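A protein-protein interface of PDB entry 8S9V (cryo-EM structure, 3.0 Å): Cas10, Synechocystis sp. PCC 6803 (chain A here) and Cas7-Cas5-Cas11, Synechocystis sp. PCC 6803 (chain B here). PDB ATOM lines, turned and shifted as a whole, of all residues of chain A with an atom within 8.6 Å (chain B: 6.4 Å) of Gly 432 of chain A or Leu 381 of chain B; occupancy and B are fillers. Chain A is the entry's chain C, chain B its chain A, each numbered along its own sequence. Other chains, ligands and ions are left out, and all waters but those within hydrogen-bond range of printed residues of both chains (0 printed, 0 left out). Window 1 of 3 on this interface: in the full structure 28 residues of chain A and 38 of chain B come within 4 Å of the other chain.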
ATOM      1  N   PHE A 383      -0.125 -11.897  -4.232  1.00  0.00           N
ATOM      2  CA  PHE A 383      -0.881 -12.725  -5.146  1.00  0.00           C
ATOM      3  C   PHE A 383      -2.143 -13.253  -4.467  1.00  0.00           C
ATOM      4  O   PHE A 383      -2.122 -13.571  -3.277  1.00  0.00           O
ATOM      5  CB  PHE A 383       0.006 -13.868  -5.631  1.00  0.00           C
ATOM      6  CG  PHE A 383      -0.622 -14.718  -6.672  1.00  0.00           C
ATOM      7  CD1 PHE A 383      -1.364 -15.820  -6.326  1.00  0.00           C
ATOM      8  CD2 PHE A 383      -0.504 -14.393  -7.997  1.00  0.00           C
ATOM      9  CE1 PHE A 383      -1.952 -16.581  -7.279  1.00  0.00           C
ATOM     10  CE2 PHE A 383      -1.095 -15.150  -8.941  1.00  0.00           C
ATOM     11  CZ  PHE A 383      -1.819 -16.242  -8.584  1.00  0.00           C
ATOM     12  N   VAL A 387      -6.706 -18.007  -5.419  1.00  0.00           N
ATOM     13  CA  VAL A 387      -6.061 -18.694  -6.529  1.00  0.00           C
ATOM     14  C   VAL A 387      -4.956 -19.619  -6.039  1.00  0.00           C
ATOM     15  O   VAL A 387      -4.866 -20.773  -6.457  1.00  0.00           O
ATOM     16  CB  VAL A 387      -5.520 -17.667  -7.531  1.00  0.00           C
ATOM     17  CG1 VAL A 387      -4.882 -18.361  -8.687  1.00  0.00           C
ATOM     18  CG2 VAL A 387      -6.624 -16.776  -7.997  1.00  0.00           C
ATOM     19  N   LEU A 391      -4.390 -23.913  -6.306  1.00  0.00           N
ATOM     20  CA  LEU A 391      -3.207 -24.704  -6.633  1.00  0.00           C
ATOM     21  C   LEU A 391      -2.917 -25.759  -5.580  1.00  0.00           C
ATOM     22  O   LEU A 391      -2.749 -26.936  -5.902  1.00  0.00           O
ATOM     23  CB  LEU A 391      -1.991 -23.806  -6.782  1.00  0.00           C
ATOM     24  CG  LEU A 391      -1.373 -23.573  -8.141  1.00  0.00           C
ATOM     25  CD1 LEU A 391      -0.326 -22.504  -8.032  1.00  0.00           C
ATOM     26  CD2 LEU A 391      -0.755 -24.844  -8.634  1.00  0.00           C
ATOM     27  N   LEU A 427       5.389 -20.053  -7.675  1.00  0.00           N
ATOM     28  CA  LEU A 427       4.653 -19.523  -8.823  1.00  0.00           C
ATOM     29  C   LEU A 427       5.431 -18.622  -9.798  1.00  0.00           C
ATOM     30  O   LEU A 427       5.478 -18.920 -10.995  1.00  0.00           O
ATOM     31  CB  LEU A 427       3.411 -18.819  -8.302  1.00  0.00           C
ATOM     32  CG  LEU A 427       2.405 -18.412  -9.346  1.00  0.00           C
ATOM     33  CD1 LEU A 427       1.976 -19.608 -10.076  1.00  0.00           C
ATOM     34  CD2 LEU A 427       1.260 -17.871  -8.603  1.00  0.00           C
ATOM     35  N   ASP A 429       4.678 -15.906 -11.257  1.00  0.00           N
ATOM     36  CA  ASP A 429       3.749 -15.525 -12.312  1.00  0.00           C
ATOM     37  C   ASP A 429       2.769 -14.540 -11.732  1.00  0.00           C
ATOM     38  O   ASP A 429       2.631 -14.426 -10.516  1.00  0.00           O
ATOM     39  CB  ASP A 429       2.936 -16.691 -12.867  1.00  0.00           C
ATOM     40  CG  ASP A 429       3.504 -17.256 -14.136  1.00  0.00           C
ATOM     41  OD1 ASP A 429       4.515 -16.730 -14.629  1.00  0.00           O
ATOM     42  OD2 ASP A 429       2.926 -18.235 -14.649  1.00  0.00           O
ATOM     43  N   SER A 430       2.092 -13.818 -12.610  1.00  0.00           N
ATOM     44  CA  SER A 430       1.142 -12.806 -12.186  1.00  0.00           C
ATOM     45  C   SER A 430      -0.284 -13.229 -12.447  1.00  0.00           C
ATOM     46  O   SER A 430      -1.166 -12.891 -11.675  1.00  0.00           O
ATOM     47  CB  SER A 430       1.417 -11.480 -12.889  1.00  0.00           C
ATOM     48  OG  SER A 430       2.759 -11.083 -12.729  1.00  0.00           O
ATOM     49  N   SER A 431      -0.534 -13.936 -13.538  1.00  0.00           N
ATOM     50  CA  SER A 431      -1.846 -14.510 -13.761  1.00  0.00           C
ATOM     51  C   SER A 431      -1.717 -15.674 -14.724  1.00  0.00           C
ATOM     52  O   SER A 431      -0.911 -15.631 -15.650  1.00  0.00           O
ATOM     53  CB  SER A 431      -2.811 -13.477 -14.310  1.00  0.00           C
ATOM     54  OG  SER A 431      -2.421 -13.104 -15.607  1.00  0.00           O
ATOM     55  N   GLY A 432      -2.505 -16.711 -14.488  1.00  0.00           N
ATOM     56  CA  GLY A 432      -2.635 -17.857 -15.366  1.00  0.00           C
ATOM     57  C   GLY A 432      -3.035 -19.016 -14.487  1.00  0.00           C
ATOM     58  O   GLY A 432      -4.174 -19.482 -14.510  1.00  0.00           O
ATOM     59  N   ILE A 433      -2.081 -19.464 -13.676  1.00  0.00           N
ATOM     60  CA  ILE A 433      -2.334 -20.423 -12.609  1.00  0.00           C
ATOM     61  C   ILE A 433      -3.274 -21.554 -12.999  1.00  0.00           C
ATOM     62  O   ILE A 433      -4.384 -21.657 -12.472  1.00  0.00           O
ATOM     63  CB  ILE A 433      -2.808 -19.694 -11.347  1.00  0.00           C
ATOM     64  CG1 ILE A 433      -2.778 -18.202 -11.610  1.00  0.00           C
ATOM     65  CG2 ILE A 433      -1.908 -20.019 -10.192  1.00  0.00           C
ATOM     66  CD1 ILE A 433      -1.402 -17.644 -11.509  1.00  0.00           C
ATOM     67  N   ASP A 434      -2.855 -22.376 -13.957  1.00  0.00           N
ATOM     68  CA  ASP A 434      -3.582 -23.585 -14.313  1.00  0.00           C
ATOM     69  C   ASP A 434      -2.560 -24.694 -14.179  1.00  0.00           C
ATOM     70  O   ASP A 434      -1.608 -24.762 -14.955  1.00  0.00           O
ATOM     71  CB  ASP A 434      -4.139 -23.528 -15.729  1.00  0.00           C
ATOM     72  CG  ASP A 434      -5.132 -24.636 -16.001  1.00  0.00           C
ATOM     73  OD1 ASP A 434      -5.483 -25.356 -15.046  1.00  0.00           O
ATOM     74  OD2 ASP A 434      -5.569 -24.790 -17.158  1.00  0.00           O
ATOM     75  N   PHE A 435      -2.765 -25.559 -13.193  1.00  0.00           N
ATOM     76  CA  PHE A 435      -1.867 -26.682 -12.976  1.00  0.00           C
ATOM     77  C   PHE A 435      -1.561 -27.435 -14.265  1.00  0.00           C
ATOM     78  O   PHE A 435      -0.424 -27.853 -14.493  1.00  0.00           O
ATOM     79  CB  PHE A 435      -2.468 -27.601 -11.919  1.00  0.00           C
ATOM     80  CG  PHE A 435      -1.551 -28.680 -11.465  1.00  0.00           C
ATOM     81  CD1 PHE A 435      -0.384 -28.367 -10.823  1.00  0.00           C
ATOM     82  CD2 PHE A 435      -1.857 -29.999 -11.661  1.00  0.00           C
ATOM     83  CE1 PHE A 435       0.451 -29.342 -10.405  1.00  0.00           C
ATOM     84  CE2 PHE A 435      -1.012 -30.972 -11.236  1.00  0.00           C
ATOM     85  CZ  PHE A 435       0.137 -30.642 -10.609  1.00  0.00           C
ATOM     86  N   ASP A 436      -2.556 -27.604 -15.130  1.00  0.00           N
ATOM     87  CA  ASP A 436      -2.328 -28.311 -16.385  1.00  0.00           C
ATOM     88  C   ASP A 436      -1.446 -27.533 -17.349  1.00  0.00           C
ATOM     89  O   ASP A 436      -0.565 -28.112 -17.986  1.00  0.00           O
ATOM     90  CB  ASP A 436      -3.664 -28.630 -17.025  1.00  0.00           C
ATOM     91  CG  ASP A 436      -4.441 -29.619 -16.229  1.00  0.00           C
ATOM     92  OD1 ASP A 436      -3.850 -30.221 -15.319  1.00  0.00           O
ATOM     93  OD2 ASP A 436      -5.644 -29.793 -16.498  1.00  0.00           O
ATOM     94  N   ARG A 437      -1.680 -26.235 -17.503  1.00  0.00           N
ATOM     95  CA  ARG A 437      -0.750 -25.423 -18.273  1.00  0.00           C
ATOM     96  C   ARG A 437       0.609 -25.365 -17.607  1.00  0.00           C
ATOM     97  O   ARG A 437       1.641 -25.449 -18.274  1.00  0.00           O
ATOM     98  CB  ARG A 437      -1.282 -24.010 -18.481  1.00  0.00           C
ATOM     99  CG  ARG A 437      -2.263 -23.812 -19.625  1.00  0.00           C
ATOM    100  CD  ARG A 437      -3.680 -24.175 -19.272  1.00  0.00           C
ATOM    101  NE  ARG A 437      -4.612 -23.693 -20.291  1.00  0.00           N
ATOM    102  CZ  ARG A 437      -5.936 -23.755 -20.187  1.00  0.00           C
ATOM    103  NH1 ARG A 437      -6.698 -23.270 -21.156  1.00  0.00           N
ATOM    104  NH2 ARG A 437      -6.503 -24.262 -19.098  1.00  0.00           N
ATOM    105  N   ILE A 438       0.629 -25.199 -16.291  1.00  0.00           N
ATOM    106  CA  ILE A 438       1.885 -25.113 -15.557  1.00  0.00           C
ATOM    107  C   ILE A 438       2.761 -26.323 -15.822  1.00  0.00           C
ATOM    108  O   ILE A 438       3.956 -26.191 -16.093  1.00  0.00           O
ATOM    109  CB  ILE A 438       1.611 -24.953 -14.055  1.00  0.00           C
ATOM    110  CG1 ILE A 438       1.215 -23.521 -13.724  1.00  0.00           C
ATOM    111  CG2 ILE A 438       2.794 -25.402 -13.270  1.00  0.00           C
ATOM    112  CD1 ILE A 438       0.577 -23.378 -12.382  1.00  0.00           C
ATOM    113  N   MET B  20       2.281 -14.635 -17.284  1.00  0.00           N
ATOM    114  CA  MET B  20       2.951 -15.923 -17.330  1.00  0.00           C
ATOM    115  C   MET B  20       4.159 -15.894 -18.265  1.00  0.00           C
ATOM    116  O   MET B  20       4.351 -14.953 -19.026  1.00  0.00           O
ATOM    117  CB  MET B  20       1.937 -16.979 -17.724  1.00  0.00           C
ATOM    118  CG  MET B  20       1.478 -16.866 -19.118  1.00  0.00           C
ATOM    119  SD  MET B  20       0.200 -18.073 -19.363  1.00  0.00           S
ATOM    120  CE  MET B  20      -1.022 -17.354 -18.288  1.00  0.00           C
ATOM    121  N   GLN B  30       0.822 -12.475 -25.432  1.00  0.00           N
ATOM    122  CA  GLN B  30      -0.516 -12.996 -25.661  1.00  0.00           C
ATOM    123  C   GLN B  30      -0.609 -13.677 -27.015  1.00  0.00           C
ATOM    124  O   GLN B  30      -0.163 -13.123 -28.015  1.00  0.00           O
ATOM    125  CB  GLN B  30      -1.493 -11.822 -25.608  1.00  0.00           C
ATOM    126  CG  GLN B  30      -2.304 -11.683 -24.355  1.00  0.00           C
ATOM    127  CD  GLN B  30      -3.421 -12.656 -24.307  1.00  0.00           C
ATOM    128  OE1 GLN B  30      -4.361 -12.574 -25.090  1.00  0.00           O
ATOM    129  NE2 GLN B  30      -3.325 -13.623 -23.405  1.00  0.00           N
ATOM    130  N   VAL B 268     -11.475 -12.571 -10.216  1.00  0.00           N
ATOM    131  CA  VAL B 268     -11.677 -13.405 -11.393  1.00  0.00           C
ATOM    132  C   VAL B 268     -13.156 -13.682 -11.557  1.00  0.00           C
ATOM    133  O   VAL B 268     -13.782 -14.250 -10.664  1.00  0.00           O
ATOM    134  CB  VAL B 268     -10.893 -14.712 -11.280  1.00  0.00           C
ATOM    135  CG1 VAL B 268     -11.176 -15.319  -9.988  1.00  0.00           C
ATOM    136  CG2 VAL B 268     -11.313 -15.661 -12.344  1.00  0.00           C
ATOM    137  N   VAL B 269     -13.701 -13.324 -12.718  1.00  0.00           N
ATOM    138  CA  VAL B 269     -15.033 -13.747 -13.145  1.00  0.00           C
ATOM    139  C   VAL B 269     -14.977 -15.166 -13.681  1.00  0.00           C
ATOM    140  O   VAL B 269     -14.244 -15.449 -14.627  1.00  0.00           O
ATOM    141  CB  VAL B 269     -15.598 -12.799 -14.200  1.00  0.00           C
ATOM    142  CG1 VAL B 269     -16.964 -13.247 -14.603  1.00  0.00           C
ATOM    143  CG2 VAL B 269     -15.608 -11.396 -13.683  1.00  0.00           C
ATOM    144  N   SER B 379     -12.085 -24.086 -21.736  1.00  0.00           N
ATOM    145  CA  SER B 379     -12.212 -22.747 -21.191  1.00  0.00           C
ATOM    146  C   SER B 379     -10.824 -22.185 -20.933  1.00  0.00           C
ATOM    147  O   SER B 379      -9.868 -22.935 -20.759  1.00  0.00           O
ATOM    148  CB  SER B 379     -13.031 -22.769 -19.913  1.00  0.00           C
ATOM    149  OG  SER B 379     -13.163 -21.479 -19.379  1.00  0.00           O
ATOM    150  N   GLU B 380     -10.715 -20.861 -20.934  1.00  0.00           N
ATOM    151  CA  GLU B 380      -9.432 -20.182 -20.827  1.00  0.00           C
ATOM    152  C   GLU B 380      -9.573 -18.961 -19.930  1.00  0.00           C
ATOM    153  O   GLU B 380     -10.650 -18.387 -19.822  1.00  0.00           O
ATOM    154  CB  GLU B 380      -8.970 -19.787 -22.226  1.00  0.00           C
ATOM    155  CG  GLU B 380      -7.624 -19.157 -22.331  1.00  0.00           C
ATOM    156  CD  GLU B 380      -6.537 -20.037 -21.799  1.00  0.00           C
ATOM    157  OE1 GLU B 380      -5.986 -20.832 -22.586  1.00  0.00           O
ATOM    158  OE2 GLU B 380      -6.229 -19.948 -20.591  1.00  0.00           O
ATOM    159  N   LEU B 381      -8.491 -18.573 -19.263  1.00  0.00           N
ATOM    160  CA  LEU B 381      -8.499 -17.433 -18.352  1.00  0.00           C
ATOM    161  C   LEU B 381      -7.794 -16.253 -18.999  1.00  0.00           C
ATOM    162  O   LEU B 381      -6.619 -16.357 -19.350  1.00  0.00           O
ATOM    163  CB  LEU B 381      -7.821 -17.785 -17.032  1.00  0.00           C
ATOM    164  CG  LEU B 381      -7.903 -16.733 -15.934  1.00  0.00           C
ATOM    165  CD1 LEU B 381      -9.234 -16.841 -15.254  1.00  0.00           C
ATOM    166  CD2 LEU B 381      -6.802 -16.874 -14.938  1.00  0.00           C
ATOM    167  N   PHE B 382      -8.503 -15.137 -19.150  1.00  0.00           N
ATOM    168  CA  PHE B 382      -7.970 -13.919 -19.748  1.00  0.00           C
ATOM    169  C   PHE B 382      -7.817 -12.851 -18.680  1.00  0.00           C
ATOM    170  O   PHE B 382      -8.785 -12.525 -18.001  1.00  0.00           O
ATOM    171  CB  PHE B 382      -8.896 -13.445 -20.856  1.00  0.00           C
ATOM    172  CG  PHE B 382      -9.001 -14.406 -21.984  1.00  0.00           C
ATOM    173  CD1 PHE B 382      -9.918 -15.421 -21.946  1.00  0.00           C
ATOM    174  CD2 PHE B 382      -8.174 -14.321 -23.057  1.00  0.00           C
ATOM    175  CE1 PHE B 382     -10.012 -16.304 -22.959  1.00  0.00           C
ATOM    176  CE2 PHE B 382      -8.274 -15.207 -24.060  1.00  0.00           C
ATOM    177  CZ  PHE B 382      -9.190 -16.200 -24.007  1.00  0.00           C
ATOM    178  N   THR B 383      -6.622 -12.296 -18.535  1.00  0.00           N
ATOM    179  CA  THR B 383      -6.349 -11.284 -17.524  1.00  0.00           C
ATOM    180  C   THR B 383      -6.142  -9.913 -18.146  1.00  0.00           C
ATOM    181  O   THR B 383      -5.391  -9.775 -19.112  1.00  0.00           O
ATOM    182  CB  THR B 383      -5.132 -11.665 -16.697  1.00  0.00           C
ATOM    183  OG1 THR B 383      -5.366 -12.925 -16.072  1.00  0.00           O
ATOM    184  CG2 THR B 383      -4.859 -10.645 -15.648  1.00  0.00           C
ATOM    185  N   SER B 403      -9.749 -10.755 -14.182  1.00  0.00           N
ATOM    186  CA  SER B 403      -9.656 -11.866 -15.098  1.00  0.00           C
ATOM    187  C   SER B 403     -11.045 -12.329 -15.456  1.00  0.00           C
ATOM    188  O   SER B 403     -11.956 -12.270 -14.637  1.00  0.00           O
ATOM    189  CB  SER B 403      -8.913 -13.025 -14.474  1.00  0.00           C
ATOM    190  OG  SER B 403      -7.641 -12.628 -14.020  1.00  0.00           O
ATOM    191  N   TYR B 404     -11.204 -12.768 -16.691  1.00  0.00           N
ATOM    192  CA  TYR B 404     -12.384 -13.483 -17.137  1.00  0.00           C
ATOM    193  C   TYR B 404     -11.996 -14.902 -17.491  1.00  0.00           C
ATOM    194  O   TYR B 404     -11.055 -15.098 -18.255  1.00  0.00           O
ATOM    195  CB  TYR B 404     -12.999 -12.813 -18.353  1.00  0.00           C
ATOM    196  CG  TYR B 404     -13.461 -11.409 -18.168  1.00  0.00           C
ATOM    197  CD1 TYR B 404     -13.810 -10.928 -16.942  1.00  0.00           C
ATOM    198  CD2 TYR B 404     -13.622 -10.588 -19.244  1.00  0.00           C
ATOM    199  CE1 TYR B 404     -14.247  -9.658 -16.798  1.00  0.00           C
ATOM    200  CE2 TYR B 404     -14.073  -9.327 -19.106  1.00  0.00           C
ATOM    201  CZ  TYR B 404     -14.378  -8.864 -17.888  1.00  0.00           C
ATOM    202  OH  TYR B 404     -14.847  -7.590 -17.780  1.00  0.00           O
ATOM    203  N   GLU B 405     -12.698 -15.888 -16.945  1.00  0.00           N
ATOM    204  CA  GLU B 405     -12.798 -17.160 -17.645  1.00  0.00           C
ATOM    205  C   GLU B 405     -13.712 -17.016 -18.841  1.00  0.00           C
ATOM    206  O   GLU B 405     -14.760 -16.386 -18.754  1.00  0.00           O
ATOM    207  CB  GLU B 405     -13.311 -18.259 -16.743  1.00  0.00           C
ATOM    208  CG  GLU B 405     -12.383 -18.580 -15.638  1.00  0.00           C
ATOM    209  CD  GLU B 405     -12.876 -19.725 -14.813  1.00  0.00           C
ATOM    210  OE1 GLU B 405     -14.063 -20.070 -14.953  1.00  0.00           O
ATOM    211  OE2 GLU B 405     -12.088 -20.266 -14.009  1.00  0.00           O
ATOM    212  N   ALA B 406     -13.365 -17.684 -19.931  1.00  0.00           N
ATOM    213  CA  ALA B 406     -14.191 -17.667 -21.117  1.00  0.00           C
ATOM    214  C   ALA B 406     -14.209 -19.033 -21.774  1.00  0.00           C
ATOM    215  O   ALA B 406     -13.253 -19.793 -21.676  1.00  0.00           O
ATOM    216  CB  ALA B 406     -13.663 -16.632 -22.086  1.00  0.00           C
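NH1 of Arg 437 of chain A sits at hydrogen-bond distance from O of Ser 379 of chain B, 3.2 Å away.
The guanidinium group (NH1) of Arg 437 of chain A lies within salt-bridge range of the side-chain carboxylate (OE1) of Glu 380 of chain B.
The side-chain hydroxyl (OG1) of Thr 383 of chain B sits at hydrogen-bond distance from the side-chain hydroxyl (OG) of Ser 431 of chain A, at 3.0 Å.
The side-chain hydroxyl (OG) of Ser 379 of chain B sits at hydrogen-bond distance from the backbone carbonyl oxygen (O) of Ala 406 of chain B (2.9 Å).
N of Ala 406 of chain B sits at hydrogen-bond distance from O of Glu 380 of chain B, 2.8 Å away.
The side-chain hydroxyl of Ser 403 of chain B is in hydrogen-bond range of the side-chain hydroxyl of Thr 383 of chain B, at 3.1 Å.
OD2 of Asp 434 of chain A lies within salt-bridge range of NE of Arg 437 of chain A.
Asp 429 of chain A touches Met 20 of chain B.
Met 20 of chain B touches Ser 431 of chain A (CE to O, 3.2 Å).
Met 20 of chain B touches Gly 432 of chain A.
CD2 of Leu 381 of chain B touches O of Gly 432 of chain A, at 3.7 Å.
Of the printed residues of chain B, Ser 431 of chain A touches Met 20 and Thr 383.
Gly 432 of chain A touches just these residues of chain B: Met 20 and Leu 381.
Gln 30 of chain B touches none of the printed residues of chain A.
Printed residues of chain A within 4 Å of Glu 380 of chain B: Arg 437.
Leu 381 of chain B touches one residue of chain A.
The nearest residue of chain B that does not touch Gly 432 of chain A is Thr 383 of chain B (5.0 Å).
Of the 14 printed residues of chain A, 4 touch a printed residue of chain B.
Printed residues of chain A that touch a printed residue of chain B: Asp 429, Ser 431, Gly 432 and Arg 437.
Hydrophobic or aromatic side chains of chain B that line the printed part of chain A: Met 20 and Leu 381.
Among the printed residues, Asp or Glu carboxylates within 4 Å of a Lys or Arg side-chain nitrogen of the other chain: Arg 437 of chain A with Glu 380 of chain B.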
